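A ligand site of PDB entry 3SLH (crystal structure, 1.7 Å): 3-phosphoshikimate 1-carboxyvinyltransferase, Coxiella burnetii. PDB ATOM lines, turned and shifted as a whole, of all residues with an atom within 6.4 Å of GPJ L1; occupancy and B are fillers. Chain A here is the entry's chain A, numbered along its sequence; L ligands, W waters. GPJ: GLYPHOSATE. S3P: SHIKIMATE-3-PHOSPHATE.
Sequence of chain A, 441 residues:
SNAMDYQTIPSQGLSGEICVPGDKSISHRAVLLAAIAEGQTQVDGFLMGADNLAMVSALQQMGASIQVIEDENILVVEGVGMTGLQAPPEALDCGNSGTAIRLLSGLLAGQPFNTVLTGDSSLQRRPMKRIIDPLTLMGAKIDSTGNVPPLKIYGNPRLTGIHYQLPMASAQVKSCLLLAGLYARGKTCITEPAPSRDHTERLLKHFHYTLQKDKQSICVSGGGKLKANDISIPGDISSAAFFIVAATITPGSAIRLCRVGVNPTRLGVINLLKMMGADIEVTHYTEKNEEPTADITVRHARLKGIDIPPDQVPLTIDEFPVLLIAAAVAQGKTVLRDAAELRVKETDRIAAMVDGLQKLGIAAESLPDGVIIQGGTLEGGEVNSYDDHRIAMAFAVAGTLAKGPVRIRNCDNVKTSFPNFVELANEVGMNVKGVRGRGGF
O of Ser 238 is in hydrogen-bond range of NH1 of Arg 390 (3.5 Å).
OG1 of Thr 99 lies within hydrogen-bond range of NE2 of Gln 172, at 3.1 Å.
The guanidinium group of Arg 349 lies within salt-bridge range of the side-chain carboxylate of Glu 346, 3.3 Å away.
The backbone carbonyl oxygen (O) of Lys 345 sits close to the guanidinium group (NE) of Arg 126.
The side-chain carboxylate of Asp 318 is in salt-bridge range of the guanidinium group of Arg 349, 3.6 Å away.
The guanidinium group of Arg 349 lies within hydrogen-bond range of a ring nitrogen (NE2) of His 389.
The side-chain amide oxygen (OE1) of Gln 172 sits at hydrogen-bond distance from the guanidinium group (NH1) of Arg 102, 2.7 Å away.
OG of Ser 97 lies within hydrogen-bond range of N of Ala 100 (3.0 Å).
The guanidinium group (NE) of Arg 390 lies within salt-bridge range of an oxygen (O5) of GPJ L1, 2.6 Å away.
The backbone NH (N) of Thr 99 sits at hydrogen-bond distance from an oxygen (O2) of GPJ L1 (3.2 Å).
The side-chain hydroxyl (OG1) of Thr 99 is in hydrogen-bond range of an oxygen (O2) of GPJ L1.
N1 of GPJ L1 lies within salt-bridge range of OE2 of Glu 346 (2.8 Å).
An oxygen (O3) of GPJ L1 lies within salt-bridge range of the guanidinium group (NH2) of Arg 126, at 2.8 Å.
The guanidinium group (NH1) of Arg 349 is in salt-bridge range of an oxygen (O5) of GPJ L1, at 2.8 Å.
The side-chain amide nitrogen (NE2) of Gln 172 lies within hydrogen-bond range of an oxygen (O3) of GPJ L1 (2.8 Å).
The side-chain amino group of Lys 24 is in salt-bridge range of an oxygen (O4) of GPJ L1, at 2.9 Å.
The backbone NH (N) of Gly 98 lies within hydrogen-bond range of an oxygen (O1) of GPJ L1 (2.9 Å).
O4 of GPJ L1 lies close to NE2 of His 389, at 3.5 Å.
NH1 of Arg 102 lies within salt-bridge range of O3 of GPJ L1, at 3.7 Å.
N of Gln 172 lies within hydrogen-bond range of O6 of S3P L2, at 2.8 Å.
NE2 of Gln 172 lies within hydrogen-bond range of O1 of S3P L2, 3.2 Å away.
The side-chain carboxylate of Asp 318 is in hydrogen-bond range of an oxygen (O3) of S3P L2 (2.7 Å).
NZ of Lys 345 is in salt-bridge range of O8 of S3P L2 (3.3 Å).
OD1 of Asp 318 sits close to O5 of GPJ L1, 3.3 Å away.
Residues that only touch GPJ L1: Asn 96 (3.6 Å) and Ser 97 (3.9 Å).
Hydrophobic or aromatic side chains that line GPJ L1: His 389.
Within 4 Å of GPJ L1: Lys 24, Asn 96, Ser 97, Gly 98, Thr 99, Arg 102, Arg 126, Gln 172, Asp 318, Glu 346, Arg 349, His 389 and Arg 390.
Along chain A the residues within 4 Å of GPJ L1 span positions 24 to 390.
Water W1 lies within hydrogen-bond range of the side-chain carboxylate (OD2) of Asp 51, the side-chain hydroxyl (OG) of Ser 97, an oxygen (O2) of GPJ L1 and a ring nitrogen (NE2) of His 28.
An oxygen (O3) of S3P L2 sits at hydrogen-bond distance from a nitrogen (N1) of GPJ L1 (2.9 Å).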
ATOM      1  N   LYS A  24     -36.885 -17.277 -32.388  1.00  0.00           N
ATOM      2  CA  LYS A  24     -36.422 -18.685 -32.326  1.00  0.00           C
ATOM      3  C   LYS A  24     -36.734 -19.328 -30.961  1.00  0.00           C
ATOM      4  O   LYS A  24     -37.251 -20.453 -30.904  1.00  0.00           O
ATOM      5  CB  LYS A  24     -34.924 -18.713 -32.636  1.00  0.00           C
ATOM      6  CG  LYS A  24     -34.309 -20.092 -32.610  1.00  0.00           C
ATOM      7  CD  LYS A  24     -32.936 -20.122 -33.270  1.00  0.00           C
ATOM      8  CE  LYS A  24     -31.918 -19.170 -32.656  1.00  0.00           C
ATOM      9  NZ  LYS A  24     -31.534 -19.504 -31.282  1.00  0.00           N
ATOM     10  N   HIS A  28     -39.550 -22.399 -30.325  1.00  0.00           N
ATOM     11  CA  HIS A  28     -39.212 -23.704 -29.809  1.00  0.00           C
ATOM     12  C   HIS A  28     -40.195 -24.120 -28.713  1.00  0.00           C
ATOM     13  O   HIS A  28     -40.722 -25.230 -28.707  1.00  0.00           O
ATOM     14  CB  HIS A  28     -37.798 -23.757 -29.219  1.00  0.00           C
ATOM     15  CG  HIS A  28     -36.689 -23.925 -30.232  1.00  0.00           C
ATOM     16  ND1 HIS A  28     -36.581 -25.029 -31.051  1.00  0.00           N
ATOM     17  CD2 HIS A  28     -35.547 -23.228 -30.392  1.00  0.00           C
ATOM     18  CE1 HIS A  28     -35.459 -24.945 -31.751  1.00  0.00           C
ATOM     19  NE2 HIS A  28     -34.811 -23.855 -31.368  1.00  0.00           N
ATOM     20  N   ASP A  51     -33.276 -24.749 -37.134  1.00  0.00           N
ATOM     21  CA  ASP A  51     -33.302 -25.134 -35.724  1.00  0.00           C
ATOM     22  C   ASP A  51     -34.740 -25.458 -35.288  1.00  0.00           C
ATOM     23  O   ASP A  51     -35.006 -26.510 -34.711  1.00  0.00           O
ATOM     24  CB  ASP A  51     -32.724 -24.052 -34.820  1.00  0.00           C
ATOM     25  CG  ASP A  51     -31.203 -24.023 -34.808  1.00  0.00           C
ATOM     26  OD1 ASP A  51     -30.589 -24.758 -35.600  1.00  0.00           O
ATOM     27  OD2 ASP A  51     -30.644 -23.245 -34.012  1.00  0.00           O
ATOM     28  N   ASN A  96     -28.353 -28.070 -35.378  1.00  0.00           N
ATOM     29  CA  ASN A  96     -27.396 -27.148 -34.767  1.00  0.00           C
ATOM     30  C   ASN A  96     -27.924 -26.622 -33.441  1.00  0.00           C
ATOM     31  O   ASN A  96     -27.261 -25.816 -32.801  1.00  0.00           O
ATOM     32  CB  ASN A  96     -27.259 -25.949 -35.711  1.00  0.00           C
ATOM     33  CG  ASN A  96     -26.030 -25.082 -35.437  1.00  0.00           C
ATOM     34  OD1 ASN A  96     -26.167 -23.865 -35.220  1.00  0.00           O
ATOM     35  ND2 ASN A  96     -24.860 -25.676 -35.497  1.00  0.00           N
ATOM     36  N   SER A  97     -29.105 -27.093 -33.030  1.00  0.00           N
ATOM     37  CA  SER A  97     -29.854 -26.450 -31.919  1.00  0.00           C
ATOM     38  C   SER A  97     -29.663 -26.942 -30.499  1.00  0.00           C
ATOM     39  O   SER A  97     -30.196 -27.980 -30.096  1.00  0.00           O
ATOM     40  CB  SER A  97     -31.372 -26.521 -32.232  1.00  0.00           C
ATOM     41  OG  SER A  97     -32.168 -25.797 -31.275  1.00  0.00           O
ATOM     42  N   GLY A  98     -28.919 -26.156 -29.706  1.00  0.00           N
ATOM     43  CA  GLY A  98     -28.767 -26.451 -28.294  1.00  0.00           C
ATOM     44  C   GLY A  98     -30.093 -26.300 -27.569  1.00  0.00           C
ATOM     45  O   GLY A  98     -30.445 -27.140 -26.720  1.00  0.00           O
ATOM     46  N   THR A  99     -30.904 -25.287 -27.928  1.00  0.00           N
ATOM     47  CA  THR A  99     -32.192 -25.118 -27.287  1.00  0.00           C
ATOM     48  C   THR A  99     -33.046 -26.354 -27.467  1.00  0.00           C
ATOM     49  O   THR A  99     -33.665 -26.855 -26.524  1.00  0.00           O
ATOM     50  CB  THR A  99     -32.962 -23.853 -27.846  1.00  0.00           C
ATOM     51  OG1 THR A  99     -32.151 -22.694 -27.682  1.00  0.00           O
ATOM     52  CG2 THR A  99     -34.320 -23.672 -27.133  1.00  0.00           C
ATOM     53  N   ALA A 100     -33.078 -26.890 -28.687  1.00  0.00           N
ATOM     54  CA  ALA A 100     -33.879 -28.077 -28.929  1.00  0.00           C
ATOM     55  C   ALA A 100     -33.403 -29.253 -28.104  1.00  0.00           C
ATOM     56  O   ALA A 100     -34.227 -29.922 -27.448  1.00  0.00           O
ATOM     57  CB  ALA A 100     -33.874 -28.452 -30.414  1.00  0.00           C
ATOM     58  N   ARG A 102     -31.624 -29.388 -25.332  1.00  0.00           N
ATOM     59  CA  ARG A 102     -31.751 -29.177 -23.907  1.00  0.00           C
ATOM     60  C   ARG A 102     -33.183 -29.152 -23.450  1.00  0.00           C
ATOM     61  O   ARG A 102     -33.478 -29.759 -22.423  1.00  0.00           O
ATOM     62  CB  ARG A 102     -30.935 -27.969 -23.445  1.00  0.00           C
ATOM     63  CG  ARG A 102     -29.455 -28.120 -23.766  1.00  0.00           C
ATOM     64  CD  ARG A 102     -28.652 -27.185 -22.950  1.00  0.00           C
ATOM     65  NE  ARG A 102     -27.200 -27.170 -23.202  1.00  0.00           N
ATOM     66  CZ  ARG A 102     -26.545 -26.252 -23.904  1.00  0.00           C
ATOM     67  NH1 ARG A 102     -27.193 -25.268 -24.557  1.00  0.00           N
ATOM     68  NH2 ARG A 102     -25.226 -26.312 -23.993  1.00  0.00           N
ATOM     69  N   LEU A 123     -23.098 -29.033 -32.430  1.00  0.00           N
ATOM     70  CA  LEU A 123     -23.927 -29.361 -31.278  1.00  0.00           C
ATOM     71  C   LEU A 123     -23.306 -30.471 -30.446  1.00  0.00           C
ATOM     72  O   LEU A 123     -23.385 -30.450 -29.225  1.00  0.00           O
ATOM     73  CB  LEU A 123     -25.341 -29.722 -31.710  1.00  0.00           C
ATOM     74  CG  LEU A 123     -26.300 -29.961 -30.536  1.00  0.00           C
ATOM     75  CD1 LEU A 123     -26.408 -28.735 -29.633  1.00  0.00           C
ATOM     76  CD2 LEU A 123     -27.685 -30.321 -31.067  1.00  0.00           C
ATOM     77  N   ARG A 126     -21.090 -29.378 -27.590  1.00  0.00           N
ATOM     78  CA  ARG A 126     -21.589 -28.435 -26.599  1.00  0.00           C
ATOM     79  C   ARG A 126     -21.984 -29.032 -25.269  1.00  0.00           C
ATOM     80  O   ARG A 126     -22.378 -30.210 -25.192  1.00  0.00           O
ATOM     81  CB  ARG A 126     -22.603 -27.577 -27.247  1.00  0.00           C
ATOM     82  CG  ARG A 126     -21.854 -26.638 -28.242  1.00  0.00           C
ATOM     83  CD  ARG A 126     -22.811 -25.810 -28.986  1.00  0.00           C
ATOM     84  NE  ARG A 126     -23.507 -24.917 -28.081  1.00  0.00           N
ATOM     85  CZ  ARG A 126     -24.700 -24.421 -28.326  1.00  0.00           C
ATOM     86  NH1 ARG A 126     -25.338 -24.739 -29.439  1.00  0.00           N
ATOM     87  NH2 ARG A 126     -25.296 -23.615 -27.441  1.00  0.00           N
ATOM     88  N   GLN A 172     -31.909 -22.124 -20.725  1.00  0.00           N
ATOM     89  CA  GLN A 172     -32.142 -23.500 -21.182  1.00  0.00           C
ATOM     90  C   GLN A 172     -32.213 -24.492 -20.029  1.00  0.00           C
ATOM     91  O   GLN A 172     -33.055 -25.378 -20.039  1.00  0.00           O
ATOM     92  CB  GLN A 172     -31.133 -23.945 -22.230  1.00  0.00           C
ATOM     93  CG  GLN A 172     -31.265 -23.208 -23.529  1.00  0.00           C
ATOM     94  CD  GLN A 172     -30.297 -23.696 -24.565  1.00  0.00           C
ATOM     95  OE1 GLN A 172     -29.880 -24.848 -24.514  1.00  0.00           O
ATOM     96  NE2 GLN A 172     -29.933 -22.853 -25.518  1.00  0.00           N
ATOM     97  N   SER A 238     -33.247 -10.739 -31.701  1.00  0.00           N
ATOM     98  CA  SER A 238     -31.881 -11.132 -32.032  1.00  0.00           C
ATOM     99  C   SER A 238     -31.650 -10.980 -33.544  1.00  0.00           C
ATOM    100  O   SER A 238     -30.562 -10.610 -33.970  1.00  0.00           O
ATOM    101  CB  SER A 238     -31.593 -12.567 -31.544  1.00  0.00           C
ATOM    102  OG  SER A 238     -31.590 -12.609 -30.132  1.00  0.00           O
ATOM    103  N   ILE A 317     -27.003 -11.988 -24.288  1.00  0.00           N
ATOM    104  CA  ILE A 317     -26.031 -13.046 -24.624  1.00  0.00           C
ATOM    105  C   ILE A 317     -25.802 -13.331 -26.127  1.00  0.00           C
ATOM    106  O   ILE A 317     -24.665 -13.399 -26.553  1.00  0.00           O
ATOM    107  CB  ILE A 317     -26.323 -14.335 -23.801  1.00  0.00           C
ATOM    108  CG1 ILE A 317     -25.185 -15.343 -23.897  1.00  0.00           C
ATOM    109  CG2 ILE A 317     -27.645 -14.937 -24.188  1.00  0.00           C
ATOM    110  CD1 ILE A 317     -23.879 -14.822 -23.264  1.00  0.00           C
ATOM    111  N   ASP A 318     -26.874 -13.447 -26.907  1.00  0.00           N
ATOM    112  CA  ASP A 318     -26.754 -13.728 -28.320  1.00  0.00           C
ATOM    113  C   ASP A 318     -26.431 -12.512 -29.170  1.00  0.00           C
ATOM    114  O   ASP A 318     -26.067 -12.676 -30.329  1.00  0.00           O
ATOM    115  CB  ASP A 318     -28.038 -14.395 -28.814  1.00  0.00           C
ATOM    116  CG  ASP A 318     -28.237 -15.781 -28.258  1.00  0.00           C
ATOM    117  OD1 ASP A 318     -27.281 -16.380 -27.693  1.00  0.00           O
ATOM    118  OD2 ASP A 318     -29.383 -16.298 -28.413  1.00  0.00           O
ATOM    119  N   GLU A 319     -26.556 -11.311 -28.607  1.00  0.00           N
ATOM    120  CA  GLU A 319     -26.286 -10.078 -29.348  1.00  0.00           C
ATOM    121  C   GLU A 319     -24.856  -9.595 -29.178  1.00  0.00           C
ATOM    122  O   GLU A 319     -24.488  -8.616 -29.777  1.00  0.00           O
ATOM    123  CB  GLU A 319     -27.284  -8.932 -28.979  1.00  0.00           C
ATOM    124  CG  GLU A 319     -28.626  -9.101 -29.639  1.00  0.00           C
ATOM    125  CD  GLU A 319     -29.346 -10.352 -29.208  1.00  0.00           C
ATOM    126  OE1 GLU A 319     -29.384 -11.305 -29.994  1.00  0.00           O
ATOM    127  OE2 GLU A 319     -29.812 -10.409 -28.055  1.00  0.00           O
ATOM    128  N   LYS A 345     -20.957 -21.614 -27.127  1.00  0.00           N
ATOM    129  CA  LYS A 345     -22.052 -21.495 -28.066  1.00  0.00           C
ATOM    130  C   LYS A 345     -21.720 -22.294 -29.343  1.00  0.00           C
ATOM    131  O   LYS A 345     -20.857 -23.200 -29.303  1.00  0.00           O
ATOM    132  CB  LYS A 345     -22.349 -20.011 -28.305  1.00  0.00           C
ATOM    133  CG  LYS A 345     -22.756 -19.294 -27.009  1.00  0.00           C
ATOM    134  CD  LYS A 345     -24.171 -19.610 -26.594  1.00  0.00           C
ATOM    135  CE  LYS A 345     -24.510 -18.995 -25.216  1.00  0.00           C
ATOM    136  NZ  LYS A 345     -25.885 -19.388 -24.765  1.00  0.00           N
ATOM    137  N   GLU A 346     -22.455 -22.014 -30.432  1.00  0.00           N
ATOM    138  CA  GLU A 346     -22.256 -22.704 -31.743  1.00  0.00           C
ATOM    139  C   GLU A 346     -20.752 -22.764 -32.062  1.00  0.00           C
ATOM    140  O   GLU A 346     -20.235 -23.764 -32.597  1.00  0.00           O
ATOM    141  CB  GLU A 346     -23.051 -22.030 -32.843  1.00  0.00           C
ATOM    142  CG  GLU A 346     -24.599 -22.184 -32.752  1.00  0.00           C
ATOM    143  CD  GLU A 346     -25.322 -21.174 -31.849  1.00  0.00           C
ATOM    144  OE1 GLU A 346     -24.763 -20.680 -30.855  1.00  0.00           O
ATOM    145  OE2 GLU A 346     -26.502 -20.846 -32.145  1.00  0.00           O
ATOM    146  N   ARG A 349     -17.507 -17.789 -29.298  1.00  0.00           N
ATOM    147  CA  ARG A 349     -17.828 -16.506 -29.896  1.00  0.00           C
ATOM    148  C   ARG A 349     -16.844 -15.407 -29.546  1.00  0.00           C
ATOM    149  O   ARG A 349     -16.705 -14.464 -30.296  1.00  0.00           O
ATOM    150  CB  ARG A 349     -19.268 -16.093 -29.624  1.00  0.00           C
ATOM    151  CG  ARG A 349     -20.234 -17.029 -30.327  1.00  0.00           C
ATOM    152  CD  ARG A 349     -21.694 -16.684 -30.039  1.00  0.00           C
ATOM    153  NE  ARG A 349     -22.585 -17.265 -31.035  1.00  0.00           N
ATOM    154  CZ  ARG A 349     -23.908 -17.134 -31.084  1.00  0.00           C
ATOM    155  NH1 ARG A 349     -24.603 -16.522 -30.134  1.00  0.00           N
ATOM    156  NH2 ARG A 349     -24.573 -17.635 -32.108  1.00  0.00           N
ATOM    157  N   ASP A 388     -20.851 -20.327 -37.421  1.00  0.00           N
ATOM    158  CA  ASP A 388     -21.802 -19.729 -36.449  1.00  0.00           C
ATOM    159  C   ASP A 388     -22.602 -18.625 -37.129  1.00  0.00           C
ATOM    160  O   ASP A 388     -22.064 -17.631 -37.617  1.00  0.00           O
ATOM    161  CB  ASP A 388     -20.988 -19.187 -35.263  1.00  0.00           C
ATOM    162  CG  ASP A 388     -21.847 -18.621 -34.162  1.00  0.00           C
ATOM    163  OD1 ASP A 388     -22.896 -17.965 -34.444  1.00  0.00           O
ATOM    164  OD2 ASP A 388     -21.448 -18.805 -33.009  1.00  0.00           O
ATOM    165  N   HIS A 389     -23.912 -18.835 -37.230  1.00  0.00           N
ATOM    166  CA  HIS A 389     -24.819 -17.891 -37.857  1.00  0.00           C
ATOM    167  C   HIS A 389     -24.670 -16.446 -37.427  1.00  0.00           C
ATOM    168  O   HIS A 389     -24.742 -15.525 -38.272  1.00  0.00           O
ATOM    169  CB  HIS A 389     -26.290 -18.355 -37.674  1.00  0.00           C
ATOM    170  CG  HIS A 389     -26.752 -18.469 -36.254  1.00  0.00           C
ATOM    171  ND1 HIS A 389     -27.900 -17.856 -35.802  1.00  0.00           N
ATOM    172  CD2 HIS A 389     -26.255 -19.148 -35.203  1.00  0.00           C
ATOM    173  CE1 HIS A 389     -28.083 -18.154 -34.532  1.00  0.00           C
ATOM    174  NE2 HIS A 389     -27.094 -18.935 -34.134  1.00  0.00           N
ATOM    175  N   ARG A 390     -24.474 -16.217 -36.129  1.00  0.00           N
ATOM    176  CA  ARG A 390     -24.385 -14.850 -35.643  1.00  0.00           C
ATOM    177  C   ARG A 390     -23.057 -14.200 -35.919  1.00  0.00           C
ATOM    178  O   ARG A 390     -23.007 -13.002 -36.095  1.00  0.00           O
ATOM    179  CB  ARG A 390     -24.767 -14.715 -34.189  1.00  0.00           C
ATOM    180  CG  ARG A 390     -26.226 -15.096 -33.934  1.00  0.00           C
ATOM    181  CD  ARG A 390     -26.898 -14.313 -32.806  1.00  0.00           C
ATOM    182  NE  ARG A 390     -28.148 -15.021 -32.523  1.00  0.00           N
ATOM    183  CZ  ARG A 390     -29.298 -14.893 -33.179  1.00  0.00           C
ATOM    184  NH1 ARG A 390     -29.492 -13.919 -34.044  1.00  0.00           N
ATOM    185  NH2 ARG A 390     -30.297 -15.730 -32.910  1.00  0.00           N
ATOM    186  N   SER A 417     -31.354 -19.622 -38.110  1.00  0.00           N
ATOM    187  CA  SER A 417     -32.121 -18.613 -37.374  1.00  0.00           C
ATOM    188  C   SER A 417     -32.718 -17.495 -38.228  1.00  0.00           C
ATOM    189  O   SER A 417     -33.594 -16.790 -37.749  1.00  0.00           O
ATOM    190  CB  SER A 417     -31.257 -17.942 -36.290  1.00  0.00           C
ATOM    191  OG  SER A 417     -30.275 -17.061 -36.874  1.00  0.00           O
HETATM  192  P1  GPJ L   1     -28.433 -22.751 -28.889  1.00  0.00           P
HETATM  193  O1  GPJ L   1     -27.871 -23.522 -30.103  1.00  0.00           O
HETATM  194  O2  GPJ L   1     -29.904 -22.557 -29.178  1.00  0.00           O
HETATM  195  O3  GPJ L   1     -28.046 -23.310 -27.566  1.00  0.00           O
HETATM  196  O4  GPJ L   1     -28.990 -18.218 -31.295  1.00  0.00           O
HETATM  197  O5  GPJ L   1     -27.224 -16.926 -30.980  1.00  0.00           O
HETATM  198  C1  GPJ L   1     -27.582 -21.177 -28.803  1.00  0.00           C
HETATM  199  C2  GPJ L   1     -27.301 -18.990 -29.827  1.00  0.00           C
HETATM  200  C3  GPJ L   1     -27.866 -17.989 -30.801  1.00  0.00           C
HETATM  201  N1  GPJ L   1     -27.959 -20.284 -29.876  1.00  0.00           N
HETATM  202  C1  S3P L   2     -31.982 -19.673 -25.234  1.00  0.00           C
HETATM  203  C2  S3P L   2     -31.110 -19.482 -24.216  1.00  0.00           C
HETATM  204  C3  S3P L   2     -29.679 -19.049 -24.389  1.00  0.00           C
HETATM  205  C4  S3P L   2     -29.453 -18.494 -25.817  1.00  0.00           C
HETATM  206  C5  S3P L   2     -30.146 -19.358 -26.873  1.00  0.00           C
HETATM  207  C6  S3P L   2     -31.655 -19.354 -26.676  1.00  0.00           C
HETATM  208  C7  S3P L   2     -33.300 -20.221 -24.942  1.00  0.00           C
HETATM  209  O1  S3P L   2     -28.826 -20.188 -24.065  1.00  0.00           O
HETATM  210  O2  S3P L   2     -28.053 -18.426 -26.086  1.00  0.00           O
HETATM  211  O3  S3P L   2     -29.885 -18.925 -28.236  1.00  0.00           O
HETATM  212  O4  S3P L   2     -33.558 -20.684 -23.806  1.00  0.00           O
HETATM  213  O5  S3P L   2     -34.164 -20.201 -25.858  1.00  0.00           O
HETATM  214  P1  S3P L   2     -28.319 -20.583 -22.550  1.00  0.00           P
HETATM  215  O6  S3P L   2     -29.539 -21.127 -21.820  1.00  0.00           O
HETATM  216  O7  S3P L   2     -27.802 -19.261 -21.977  1.00  0.00           O
HETATM  217  O8  S3P L   2     -27.225 -21.613 -22.767  1.00  0.00           O
HETATM  218  O   HOH W   1     -31.756 -23.128 -31.561  1.00  0.00           O
HETATM  219  O   HOH W   2     -28.025 -23.048 -33.063  1.00  0.00           O
HETATM  220  O   HOH W   3     -26.716 -22.294 -25.311  1.00  0.00           O
